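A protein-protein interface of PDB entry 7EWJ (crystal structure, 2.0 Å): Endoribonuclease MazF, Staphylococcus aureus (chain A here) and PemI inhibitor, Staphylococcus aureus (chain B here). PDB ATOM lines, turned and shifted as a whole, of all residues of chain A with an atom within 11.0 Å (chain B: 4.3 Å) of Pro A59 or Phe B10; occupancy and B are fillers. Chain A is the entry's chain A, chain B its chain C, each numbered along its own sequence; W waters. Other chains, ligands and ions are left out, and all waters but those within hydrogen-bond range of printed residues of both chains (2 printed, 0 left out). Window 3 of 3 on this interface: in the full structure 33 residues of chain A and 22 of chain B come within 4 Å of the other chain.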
ATOM      1  N   ARG A  54      15.076   8.604   6.144  1.00  0.00           N
ATOM      2  CA  ARG A  54      15.812   7.677   6.996  1.00  0.00           C
ATOM      3  C   ARG A  54      16.992   7.110   6.219  1.00  0.00           C
ATOM      4  O   ARG A  54      17.061   7.202   4.985  1.00  0.00           O
ATOM      5  CB  ARG A  54      14.907   6.552   7.495  1.00  0.00           C
ATOM      6  CG  ARG A  54      14.410   5.590   6.374  1.00  0.00           C
ATOM      7  CD  ARG A  54      13.761   4.373   7.016  1.00  0.00           C
ATOM      8  NE  ARG A  54      13.100   3.497   6.062  1.00  0.00           N
ATOM      9  CZ  ARG A  54      13.725   2.644   5.272  1.00  0.00           C
ATOM     10  NH1 ARG A  54      15.067   2.537   5.306  1.00  0.00           N
ATOM     11  NH2 ARG A  54      13.000   1.879   4.457  1.00  0.00           N
ATOM     12  N   GLY A  55      17.929   6.496   6.939  1.00  0.00           N
ATOM     13  CA  GLY A  55      19.077   5.920   6.262  1.00  0.00           C
ATOM     14  C   GLY A  55      18.728   4.584   5.613  1.00  0.00           C
ATOM     15  O   GLY A  55      17.678   3.995   5.888  1.00  0.00           O
ATOM     16  N   LEU A  56      19.641   4.109   4.765  1.00  0.00           N
ATOM     17  CA  LEU A  56      19.520   2.789   4.150  1.00  0.00           C
ATOM     18  C   LEU A  56      19.581   1.721   5.227  1.00  0.00           C
ATOM     19  O   LEU A  56      20.509   1.709   6.031  1.00  0.00           O
ATOM     20  CB  LEU A  56      20.664   2.559   3.165  1.00  0.00           C
ATOM     21  CG  LEU A  56      20.678   3.003   1.710  1.00  0.00           C
ATOM     22  CD1 LEU A  56      22.081   2.893   1.167  1.00  0.00           C
ATOM     23  CD2 LEU A  56      19.700   2.268   0.830  1.00  0.00           C
ATOM     24  N   ARG A  57      18.586   0.832   5.280  1.00  0.00           N
ATOM     25  CA  ARG A  57      18.543  -0.196   6.337  1.00  0.00           C
ATOM     26  C   ARG A  57      18.358  -1.612   5.820  1.00  0.00           C
ATOM     27  O   ARG A  57      18.653  -2.558   6.559  1.00  0.00           O
ATOM     28  CB  ARG A  57      17.394   0.048   7.346  1.00  0.00           C
ATOM     29  CG  ARG A  57      17.401   1.417   8.004  1.00  0.00           C
ATOM     30  CD  ARG A  57      16.142   1.672   8.829  1.00  0.00           C
ATOM     31  NE  ARG A  57      16.257   2.948   9.539  1.00  0.00           N
ATOM     32  CZ  ARG A  57      15.304   3.522  10.278  1.00  0.00           C
ATOM     33  NH1 ARG A  57      14.099   2.960  10.402  1.00  0.00           N
ATOM     34  NH2 ARG A  57      15.571   4.663  10.911  1.00  0.00           N
ATOM     35  N   TYR A  58      17.807  -1.789   4.626  1.00  0.00           N
ATOM     36  CA  TYR A  58      17.368  -3.078   4.111  1.00  0.00           C
ATOM     37  C   TYR A  58      17.851  -3.248   2.686  1.00  0.00           C
ATOM     38  O   TYR A  58      17.980  -2.263   1.935  1.00  0.00           O
ATOM     39  CB  TYR A  58      15.840  -3.191   4.097  1.00  0.00           C
ATOM     40  CG  TYR A  58      15.199  -2.786   5.398  1.00  0.00           C
ATOM     41  CD1 TYR A  58      15.205  -3.643   6.482  1.00  0.00           C
ATOM     42  CD2 TYR A  58      14.525  -1.559   5.515  1.00  0.00           C
ATOM     43  CE1 TYR A  58      14.568  -3.293   7.674  1.00  0.00           C
ATOM     44  CE2 TYR A  58      13.901  -1.198   6.689  1.00  0.00           C
ATOM     45  CZ  TYR A  58      13.921  -2.079   7.757  1.00  0.00           C
ATOM     46  OH  TYR A  58      13.296  -1.726   8.914  1.00  0.00           O
ATOM     47  N   PRO A  59      18.060  -4.498   2.271  1.00  0.00           N
ATOM     48  CA  PRO A  59      18.315  -4.768   0.845  1.00  0.00           C
ATOM     49  C   PRO A  59      17.159  -4.385  -0.045  1.00  0.00           C
ATOM     50  O   PRO A  59      17.343  -4.311  -1.267  1.00  0.00           O
ATOM     51  CB  PRO A  59      18.583  -6.287   0.808  1.00  0.00           C
ATOM     52  CG  PRO A  59      18.959  -6.639   2.261  1.00  0.00           C
ATOM     53  CD  PRO A  59      18.206  -5.693   3.126  1.00  0.00           C
ATOM     54  N   THR A  60      15.953  -4.189   0.510  1.00  0.00           N
ATOM     55  CA  THR A  60      14.832  -3.680  -0.285  1.00  0.00           C
ATOM     56  C   THR A  60      14.944  -2.166  -0.539  1.00  0.00           C
ATOM     57  O   THR A  60      14.255  -1.633  -1.422  1.00  0.00           O
ATOM     58  CB  THR A  60      13.521  -3.978   0.438  1.00  0.00           C
ATOM     59  OG1 THR A  60      13.597  -3.405   1.743  1.00  0.00           O
ATOM     60  CG2 THR A  60      13.258  -5.536   0.563  1.00  0.00           C
ATOM     61  N   ASP A  61      15.769  -1.466   0.234  1.00  0.00           N
ATOM     62  CA  ASP A  61      15.952  -0.015   0.076  1.00  0.00           C
ATOM     63  C   ASP A  61      16.845   0.271  -1.118  1.00  0.00           C
ATOM     64  O   ASP A  61      17.827  -0.446  -1.332  1.00  0.00           O
ATOM     65  CB  ASP A  61      16.640   0.607   1.295  1.00  0.00           C
ATOM     66  CG  ASP A  61      15.781   0.655   2.520  1.00  0.00           C
ATOM     67  OD1 ASP A  61      14.530   0.621   2.402  1.00  0.00           O
ATOM     68  OD2 ASP A  61      16.382   0.797   3.632  1.00  0.00           O
ATOM     69  N   ILE A  62      16.561   1.359  -1.851  1.00  0.00           N
ATOM     70  CA  ILE A  62      17.440   1.808  -2.942  1.00  0.00           C
ATOM     71  C   ILE A  62      17.795   3.276  -2.740  1.00  0.00           C
ATOM     72  O   ILE A  62      16.898   4.132  -2.626  1.00  0.00           O
ATOM     73  CB  ILE A  62      16.802   1.580  -4.328  1.00  0.00           C
ATOM     74  CG1 ILE A  62      16.554   0.069  -4.535  1.00  0.00           C
ATOM     75  CG2 ILE A  62      17.686   2.178  -5.471  1.00  0.00           C
ATOM     76  CD1 ILE A  62      15.740  -0.240  -5.755  1.00  0.00           C
ATOM     77  N   GLN A  63      19.103   3.578  -2.682  1.00  0.00           N
ATOM     78  CA  GLN A  63      19.525   4.977  -2.602  1.00  0.00           C
ATOM     79  C   GLN A  63      19.072   5.738  -3.847  1.00  0.00           C
ATOM     80  O   GLN A  63      19.349   5.330  -4.974  1.00  0.00           O
ATOM     81  CB  GLN A  63      21.049   5.069  -2.442  1.00  0.00           C
ATOM     82  CG  GLN A  63      21.561   6.471  -2.040  1.00  0.00           C
ATOM     83  CD  GLN A  63      21.181   6.815  -0.590  1.00  0.00           C
ATOM     84  OE1 GLN A  63      21.544   6.108   0.327  1.00  0.00           O
ATOM     85  NE2 GLN A  63      20.446   7.891  -0.396  1.00  0.00           N
ATOM     86  N   VAL A  74      16.077   7.907   0.443  1.00  0.00           N
ATOM     87  CA  VAL A  74      16.057   6.453   0.288  1.00  0.00           C
ATOM     88  C   VAL A  74      14.685   6.033  -0.240  1.00  0.00           C
ATOM     89  O   VAL A  74      13.648   6.401   0.342  1.00  0.00           O
ATOM     90  CB  VAL A  74      16.413   5.755   1.621  1.00  0.00           C
ATOM     91  CG1 VAL A  74      16.184   4.257   1.537  1.00  0.00           C
ATOM     92  CG2 VAL A  74      17.933   5.992   1.916  1.00  0.00           C
ATOM     93  N   ILE A  75      14.671   5.291  -1.354  1.00  0.00           N
ATOM     94  CA  ILE A  75      13.426   4.730  -1.892  1.00  0.00           C
ATOM     95  C   ILE A  75      13.115   3.472  -1.090  1.00  0.00           C
ATOM     96  O   ILE A  75      13.917   2.531  -1.050  1.00  0.00           O
ATOM     97  CB  ILE A  75      13.545   4.386  -3.385  1.00  0.00           C
ATOM     98  CG1 ILE A  75      13.986   5.594  -4.227  1.00  0.00           C
ATOM     99  CG2 ILE A  75      12.212   3.827  -3.946  1.00  0.00           C
ATOM    100  CD1 ILE A  75      14.674   5.113  -5.525  1.00  0.00           C
ATOM    101  N   ASP A  76      11.949   3.435  -0.476  1.00  0.00           N
ATOM    102  CA  ASP A  76      11.498   2.239   0.223  1.00  0.00           C
ATOM    103  C   ASP A  76      10.593   1.468  -0.737  1.00  0.00           C
ATOM    104  O   ASP A  76       9.451   1.875  -0.975  1.00  0.00           O
ATOM    105  CB  ASP A  76      10.770   2.642   1.497  1.00  0.00           C
ATOM    106  CG  ASP A  76      10.379   1.442   2.363  1.00  0.00           C
ATOM    107  OD1 ASP A  76      10.303   0.311   1.847  1.00  0.00           O
ATOM    108  OD2 ASP A  76      10.155   1.641   3.571  1.00  0.00           O
ATOM    109  N   THR A  77      11.091   0.358  -1.285  1.00  0.00           N
ATOM    110  CA  THR A  77      10.317  -0.341  -2.309  1.00  0.00           C
ATOM    111  C   THR A  77       9.211  -1.216  -1.724  1.00  0.00           C
ATOM    112  O   THR A  77       8.381  -1.729  -2.484  1.00  0.00           O
ATOM    113  CB  THR A  77      11.227  -1.220  -3.193  1.00  0.00           C
ATOM    114  OG1 THR A  77      11.851  -2.238  -2.400  1.00  0.00           O
ATOM    115  CG2 THR A  77      12.344  -0.361  -3.903  1.00  0.00           C
ATOM    116  N   VAL A  78       9.153  -1.348  -0.400  1.00  0.00           N
ATOM    117  CA  VAL A  78       8.151  -2.210   0.239  1.00  0.00           C
ATOM    118  C   VAL A  78       6.781  -1.536   0.330  1.00  0.00           C
ATOM    119  O   VAL A  78       5.759  -2.217   0.415  1.00  0.00           O
ATOM    120  CB  VAL A  78       8.693  -2.632   1.623  1.00  0.00           C
ATOM    121  CG1 VAL A  78       7.595  -3.326   2.497  1.00  0.00           C
ATOM    122  CG2 VAL A  78       9.894  -3.583   1.435  1.00  0.00           C
ATOM    123  N   LEU A 100      19.020   3.123 -12.535  1.00  0.00           N
ATOM    124  CA  LEU A 100      18.331   2.547 -11.381  1.00  0.00           C
ATOM    125  C   LEU A 100      16.965   1.977 -11.722  1.00  0.00           C
ATOM    126  O   LEU A 100      16.370   1.291 -10.881  1.00  0.00           O
ATOM    127  CB  LEU A 100      18.130   3.612 -10.296  1.00  0.00           C
ATOM    128  CG  LEU A 100      19.324   3.913  -9.415  1.00  0.00           C
ATOM    129  CD1 LEU A 100      18.937   5.035  -8.396  1.00  0.00           C
ATOM    130  CD2 LEU A 100      19.808   2.627  -8.748  1.00  0.00           C
ATOM    131  N   ASP A 103      16.407  -1.898 -11.534  1.00  0.00           N
ATOM    132  CA  ASP A 103      16.436  -2.335 -10.137  1.00  0.00           C
ATOM    133  C   ASP A 103      15.102  -2.106  -9.429  1.00  0.00           C
ATOM    134  O   ASP A 103      14.645  -2.975  -8.668  1.00  0.00           O
ATOM    135  CB  ASP A 103      17.547  -1.621  -9.390  1.00  0.00           C
ATOM    136  CG  ASP A 103      18.889  -2.291  -9.580  1.00  0.00           C
ATOM    137  OD1 ASP A 103      18.959  -3.292 -10.331  1.00  0.00           O
ATOM    138  OD2 ASP A 103      19.878  -1.781  -9.024  1.00  0.00           O
ATOM    139  N   ILE A 104      14.487  -0.937  -9.655  1.00  0.00           N
ATOM    140  CA  ILE A 104      13.182  -0.614  -9.062  1.00  0.00           C
ATOM    141  C   ILE A 104      12.156  -1.650  -9.482  1.00  0.00           C
ATOM    142  O   ILE A 104      11.431  -2.225  -8.653  1.00  0.00           O
ATOM    143  CB  ILE A 104      12.725   0.796  -9.504  1.00  0.00           C
ATOM    144  CG1 ILE A 104      13.639   1.911  -8.935  1.00  0.00           C
ATOM    145  CG2 ILE A 104      11.252   0.985  -9.154  1.00  0.00           C
ATOM    146  CD1 ILE A 104      13.514   2.074  -7.453  1.00  0.00           C
ATOM    147  N   LYS A 106      12.589  -4.618 -10.783  1.00  0.00           N
ATOM    148  CA  LYS A 106      12.907  -5.977 -10.362  1.00  0.00           C
ATOM    149  C   LYS A 106      12.645  -6.176  -8.877  1.00  0.00           C
ATOM    150  O   LYS A 106      12.261  -7.275  -8.470  1.00  0.00           O
ATOM    151  CB  LYS A 106      14.352  -6.338 -10.701  1.00  0.00           C
ATOM    152  CG  LYS A 106      14.578  -6.428 -12.238  1.00  0.00           C
ATOM    153  CD  LYS A 106      15.975  -6.978 -12.627  1.00  0.00           C
ATOM    154  CE  LYS A 106      17.075  -6.517 -11.702  1.00  0.00           C
ATOM    155  NZ  LYS A 106      18.466  -6.848 -12.195  1.00  0.00           N
ATOM    156  N   ALA A 107      12.836  -5.148  -8.053  1.00  0.00           N
ATOM    157  CA  ALA A 107      12.468  -5.300  -6.646  1.00  0.00           C
ATOM    158  C   ALA A 107      10.967  -5.535  -6.510  1.00  0.00           C
ATOM    159  O   ALA A 107      10.537  -6.465  -5.816  1.00  0.00           O
ATOM    160  CB  ALA A 107      12.934  -4.089  -5.829  1.00  0.00           C
ATOM    161  N   ILE A 108      10.152  -4.746  -7.224  1.00  0.00           N
ATOM    162  CA  ILE A 108       8.699  -4.894  -7.123  1.00  0.00           C
ATOM    163  C   ILE A 108       8.278  -6.305  -7.523  1.00  0.00           C
ATOM    164  O   ILE A 108       7.420  -6.929  -6.880  1.00  0.00           O
ATOM    165  CB  ILE A 108       7.969  -3.852  -8.001  1.00  0.00           C
ATOM    166  CG1 ILE A 108       8.338  -2.377  -7.630  1.00  0.00           C
ATOM    167  CG2 ILE A 108       6.476  -4.127  -7.988  1.00  0.00           C
ATOM    168  CD1 ILE A 108       8.368  -2.136  -6.195  1.00  0.00           C
ATOM    169  N   THR A 110       9.887  -8.978  -7.338  1.00  0.00           N
ATOM    170  CA  THR A 110      10.260  -9.920  -6.300  1.00  0.00           C
ATOM    171  C   THR A 110       9.212 -10.013  -5.198  1.00  0.00           C
ATOM    172  O   THR A 110       9.166 -11.044  -4.528  1.00  0.00           O
ATOM    173  CB  THR A 110      11.635  -9.538  -5.719  1.00  0.00           C
ATOM    174  OG1 THR A 110      12.591  -9.459  -6.791  1.00  0.00           O
ATOM    175  CG2 THR A 110      12.145 -10.590  -4.690  1.00  0.00           C
ATOM    176  N   TYR A 111       8.359  -8.983  -5.005  1.00  0.00           N
ATOM    177  CA  TYR A 111       7.262  -9.064  -4.023  1.00  0.00           C
ATOM    178  C   TYR A 111       6.009  -9.705  -4.587  1.00  0.00           C
ATOM    179  O   TYR A 111       5.105 -10.042  -3.820  1.00  0.00           O
ATOM    180  CB  TYR A 111       6.864  -7.662  -3.477  1.00  0.00           C
ATOM    181  CG  TYR A 111       8.080  -6.890  -3.019  1.00  0.00           C
ATOM    182  CD1 TYR A 111       9.093  -7.525  -2.284  1.00  0.00           C
ATOM    183  CD2 TYR A 111       8.251  -5.569  -3.372  1.00  0.00           C
ATOM    184  CE1 TYR A 111      10.251  -6.843  -1.905  1.00  0.00           C
ATOM    185  CE2 TYR A 111       9.393  -4.876  -2.989  1.00  0.00           C
ATOM    186  CZ  TYR A 111      10.386  -5.511  -2.260  1.00  0.00           C
ATOM    187  OH  TYR A 111      11.522  -4.791  -1.908  1.00  0.00           O
ATOM    188  N   ILE B   3      19.565  -7.758  -7.452  1.00  0.00           N
ATOM    189  CA  ILE B   3      18.807  -7.226  -6.315  1.00  0.00           C
ATOM    190  C   ILE B   3      17.712  -8.212  -5.895  1.00  0.00           C
ATOM    191  O   ILE B   3      17.449  -8.400  -4.703  1.00  0.00           O
ATOM    192  CB  ILE B   3      18.237  -5.828  -6.628  1.00  0.00           C
ATOM    193  CG1 ILE B   3      17.669  -5.207  -5.333  1.00  0.00           C
ATOM    194  CG2 ILE B   3      17.228  -5.874  -7.765  1.00  0.00           C
ATOM    195  CD1 ILE B   3      17.249  -3.762  -5.468  1.00  0.00           C
ATOM    196  N   ARG B   6      19.375 -10.732  -3.769  1.00  0.00           N
ATOM    197  CA  ARG B   6      19.720 -10.110  -2.465  1.00  0.00           C
ATOM    198  C   ARG B   6      18.469  -9.979  -1.601  1.00  0.00           C
ATOM    199  O   ARG B   6      18.541 -10.249  -0.433  1.00  0.00           O
ATOM    200  CB  ARG B   6      20.341  -8.737  -2.687  1.00  0.00           C
ATOM    201  CG  ARG B   6      21.834  -8.675  -2.427  1.00  0.00           C
ATOM    202  CD  ARG B   6      22.488  -7.450  -3.039  1.00  0.00           C
ATOM    203  NE  ARG B   6      21.620  -6.293  -3.157  1.00  0.00           N
ATOM    204  CZ  ARG B   6      21.349  -5.446  -2.175  1.00  0.00           C
ATOM    205  NH1 ARG B   6      21.951  -5.587  -1.003  1.00  0.00           N
ATOM    206  NH2 ARG B   6      20.460  -4.482  -2.362  1.00  0.00           N
ATOM    207  N   ILE B   7      17.363  -9.575  -2.191  1.00  0.00           N
ATOM    208  CA  ILE B   7      16.110  -9.476  -1.423  1.00  0.00           C
ATOM    209  C   ILE B   7      15.664 -10.862  -0.971  1.00  0.00           C
ATOM    210  O   ILE B   7      15.315 -11.083   0.189  1.00  0.00           O
ATOM    211  CB  ILE B   7      15.002  -8.783  -2.253  1.00  0.00           C
ATOM    212  CG1 ILE B   7      15.311  -7.286  -2.426  1.00  0.00           C
ATOM    213  CG2 ILE B   7      13.554  -9.040  -1.626  1.00  0.00           C
ATOM    214  CD1 ILE B   7      14.444  -6.632  -3.515  1.00  0.00           C
ATOM    215  N   LYS B   8      15.680 -11.827  -1.884  1.00  0.00           N
ATOM    216  CA  LYS B   8      15.237 -13.162  -1.522  1.00  0.00           C
ATOM    217  C   LYS B   8      16.144 -13.756  -0.454  1.00  0.00           C
ATOM    218  O   LYS B   8      15.661 -14.326   0.528  1.00  0.00           O
ATOM    219  CB  LYS B   8      15.223 -14.040  -2.772  1.00  0.00           C
ATOM    220  CG  LYS B   8      14.019 -13.805  -3.659  1.00  0.00           C
ATOM    221  CD  LYS B   8      13.832 -14.984  -4.619  1.00  0.00           C
ATOM    222  CE  LYS B   8      14.623 -14.782  -5.908  1.00  0.00           C
ATOM    223  NZ  LYS B   8      14.355 -15.930  -6.851  1.00  0.00           N
ATOM    224  N   ASN B   9      17.470 -13.625  -0.623  1.00  0.00           N
ATOM    225  CA  ASN B   9      18.374 -14.172   0.388  1.00  0.00           C
ATOM    226  C   ASN B   9      18.152 -13.499   1.733  1.00  0.00           C
ATOM    227  O   ASN B   9      18.153 -14.168   2.772  1.00  0.00           O
ATOM    228  CB  ASN B   9      19.838 -14.021  -0.040  1.00  0.00           C
ATOM    229  CG  ASN B   9      20.168 -14.894  -1.246  1.00  0.00           C
ATOM    230  OD1 ASN B   9      19.480 -15.876  -1.497  1.00  0.00           O
ATOM    231  ND2 ASN B   9      21.178 -14.512  -2.011  1.00  0.00           N
ATOM    232  N   PHE B  10      17.935 -12.179   1.727  1.00  0.00           N
ATOM    233  CA  PHE B  10      17.650 -11.458   2.968  1.00  0.00           C
ATOM    234  C   PHE B  10      16.468 -12.086   3.694  1.00  0.00           C
ATOM    235  O   PHE B  10      16.573 -12.503   4.860  1.00  0.00           O
ATOM    236  CB  PHE B  10      17.381  -9.972   2.645  1.00  0.00           C
ATOM    237  CG  PHE B  10      16.944  -9.152   3.842  1.00  0.00           C
ATOM    238  CD1 PHE B  10      17.854  -8.800   4.838  1.00  0.00           C
ATOM    239  CD2 PHE B  10      15.614  -8.743   3.974  1.00  0.00           C
ATOM    240  CE1 PHE B  10      17.454  -8.037   5.915  1.00  0.00           C
ATOM    241  CE2 PHE B  10      15.196  -7.987   5.086  1.00  0.00           C
ATOM    242  CZ  PHE B  10      16.114  -7.643   6.042  1.00  0.00           C
ATOM    243  N   PHE B  11      15.339 -12.224   2.996  1.00  0.00           N
ATOM    244  CA  PHE B  11      14.172 -12.762   3.674  1.00  0.00           C
ATOM    245  C   PHE B  11      14.356 -14.231   4.060  1.00  0.00           C
ATOM    246  O   PHE B  11      13.881 -14.652   5.127  1.00  0.00           O
ATOM    247  CB  PHE B  11      12.943 -12.574   2.802  1.00  0.00           C
ATOM    248  CG  PHE B  11      12.450 -11.132   2.789  1.00  0.00           C
ATOM    249  CD1 PHE B  11      12.247 -10.451   3.997  1.00  0.00           C
ATOM    250  CD2 PHE B  11      12.213 -10.469   1.582  1.00  0.00           C
ATOM    251  CE1 PHE B  11      11.783  -9.112   4.006  1.00  0.00           C
ATOM    252  CE2 PHE B  11      11.749  -9.101   1.576  1.00  0.00           C
ATOM    253  CZ  PHE B  11      11.552  -8.450   2.801  1.00  0.00           C
ATOM    254  N   GLN B  12      15.025 -15.022   3.218  1.00  0.00           N
ATOM    255  CA  GLN B  12      15.164 -16.443   3.550  1.00  0.00           C
ATOM    256  C   GLN B  12      16.081 -16.684   4.748  1.00  0.00           C
ATOM    257  O   GLN B  12      15.879 -17.662   5.480  1.00  0.00           O
ATOM    258  CB  GLN B  12      15.629 -17.243   2.336  1.00  0.00           C
ATOM    259  CG  GLN B  12      14.703 -17.037   1.118  1.00  0.00           C
ATOM    260  CD  GLN B  12      14.851 -18.117   0.043  1.00  0.00           C
ATOM    261  OE1 GLN B  12      14.586 -17.872  -1.136  1.00  0.00           O
ATOM    262  NE2 GLN B  12      15.280 -19.314   0.454  1.00  0.00           N
ATOM    263  N   SER B  13      17.063 -15.806   4.988  1.00  0.00           N
ATOM    264  CA  SER B  13      17.887 -15.890   6.198  1.00  0.00           C
ATOM    265  C   SER B  13      17.148 -15.503   7.475  1.00  0.00           C
ATOM    266  O   SER B  13      17.654 -15.770   8.573  1.00  0.00           O
ATOM    267  CB  SER B  13      19.098 -14.985   6.083  1.00  0.00           C
ATOM    268  OG  SER B  13      18.723 -13.687   6.518  1.00  0.00           O
ATOM    269  N   GLY B  14      15.983 -14.879   7.381  1.00  0.00           N
ATOM    270  CA  GLY B  14      15.269 -14.412   8.551  1.00  0.00           C
ATOM    271  C   GLY B  14      15.304 -12.904   8.732  1.00  0.00           C
ATOM    272  O   GLY B  14      14.816 -12.409   9.752  1.00  0.00           O
ATOM    273  N   GLY B  15      15.870 -12.167   7.783  1.00  0.00           N
ATOM    274  CA  GLY B  15      15.792 -10.715   7.832  1.00  0.00           C
ATOM    275  C   GLY B  15      14.347 -10.234   7.848  1.00  0.00           C
ATOM    276  O   GLY B  15      13.455 -10.854   7.250  1.00  0.00           O
ATOM    277  N   LYS B  16      14.114  -9.140   8.587  1.00  0.00           N
ATOM    278  CA  LYS B  16      12.770  -8.590   8.787  1.00  0.00           C
ATOM    279  C   LYS B  16      12.818  -7.118   8.410  1.00  0.00           C
ATOM    280  O   LYS B  16      13.721  -6.410   8.853  1.00  0.00           O
ATOM    281  CB  LYS B  16      12.277  -8.761  10.247  1.00  0.00           C
ATOM    282  CG  LYS B  16      12.195 -10.262  10.609  1.00  0.00           C
ATOM    283  CD  LYS B  16      11.085 -10.900   9.766  1.00  0.00           C
ATOM    284  CE  LYS B  16      10.902 -12.384  10.128  1.00  0.00           C
ATOM    285  NZ  LYS B  16       9.859 -13.099   9.342  1.00  0.00           N
HETATM  286  O   HOH W   1      20.284  -5.656  -9.456  1.00  0.00           O
HETATM  287  O   HOH W   2      19.992  -1.687  -0.562  1.00  0.00           O
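NH2 of Arg B6 sits at hydrogen-bond distance from O of Pro A59 (3.3 Å).
Among the printed residues, merely in contact across the chains: Tyr A58 with Lys B16, Pro A59 with Ile B7, Pro A59 with Phe B10, Ile A62 with Ile B3, Asp A103 with Ile B3, Lys A106 with Ile B3, Ala A107 with Ile B7, Thr A110 with Ile B7, Thr A110 with Lys B8 and Tyr A111 with Ile B7.
The backbone NH (N) of Tyr A58 sits at hydrogen-bond distance from the side-chain carboxylate (OD2) of Asp A61. O of Ile A62 lies within hydrogen-bond range of N of Ile A75 (2.8 Å). The side-chain hydroxyl of Thr A77 sits at hydrogen-bond distance from the side-chain hydroxyl of Tyr A111, at 2.6 Å. O of Lys A106 lies within hydrogen-bond range of OG1 of Thr A110, 2.8 Å away. The backbone carbonyl oxygen of Phe B10 is in hydrogen-bond range of the side-chain hydroxyl of Ser B13, at 3.0 Å. The backbone carbonyl oxygen (O) of Phe B10 lies within hydrogen-bond range of the backbone NH (N) of Gly B15, 3.0 Å away.
Hydrophobic or aromatic side chains of chain A within 4 Å of the printed part of chain B: Tyr A58, Pro A59, Ile A62, Ala A107 and Tyr A111. Hydrophobic or aromatic side chains of chain B that line the printed part of chain A: Ile B3, Ile B7 and Phe B10.
Water W2 lies within hydrogen-bond range of the backbone carbonyl oxygen (O) of Asp A61 (2.6 Å), the backbone carbonyl oxygen (O) of Tyr A58 (3.3 Å) and the guanidinium group (NH2) of Arg B6 (3.4 Å). Water W1 lies within hydrogen-bond range of the side-chain carboxylate (OD1) of Asp A103 (2.8 Å), the backbone NH (N) of Ile B3 (3.0 Å) and the side-chain amino group (NZ) of Lys A106 (3.5 Å).
Pro A59 touches just these residues of chain B: Arg B6, Ile B7 and Phe B10. Of chain A, only Pro A59 comes within 4 Å of Phe B10. Of chain A, only Pro A59, Ala A107, Thr A110 and Tyr A111 come within 4 Å of Ile B7. No residue of chain A comes within 4 Å of Ser B13. No residue of chain A comes within 4 Å of Gly B14. No residue of chain A comes within 4 Å of Gly B15. Printed residues of chain B within 4 Å of Tyr A58: Lys B16 (3.4 Å). Printed residues of chain A within 4 Å of Lys B8: Thr A110 (3.9 Å). Of the printed residues of chain B, Ala A107 touches Ile B7. Gln B12 touches none of the printed residues of chain A. The nearest residue of chain A that does not touch Phe B10 is Tyr A58 (4.1 Å).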
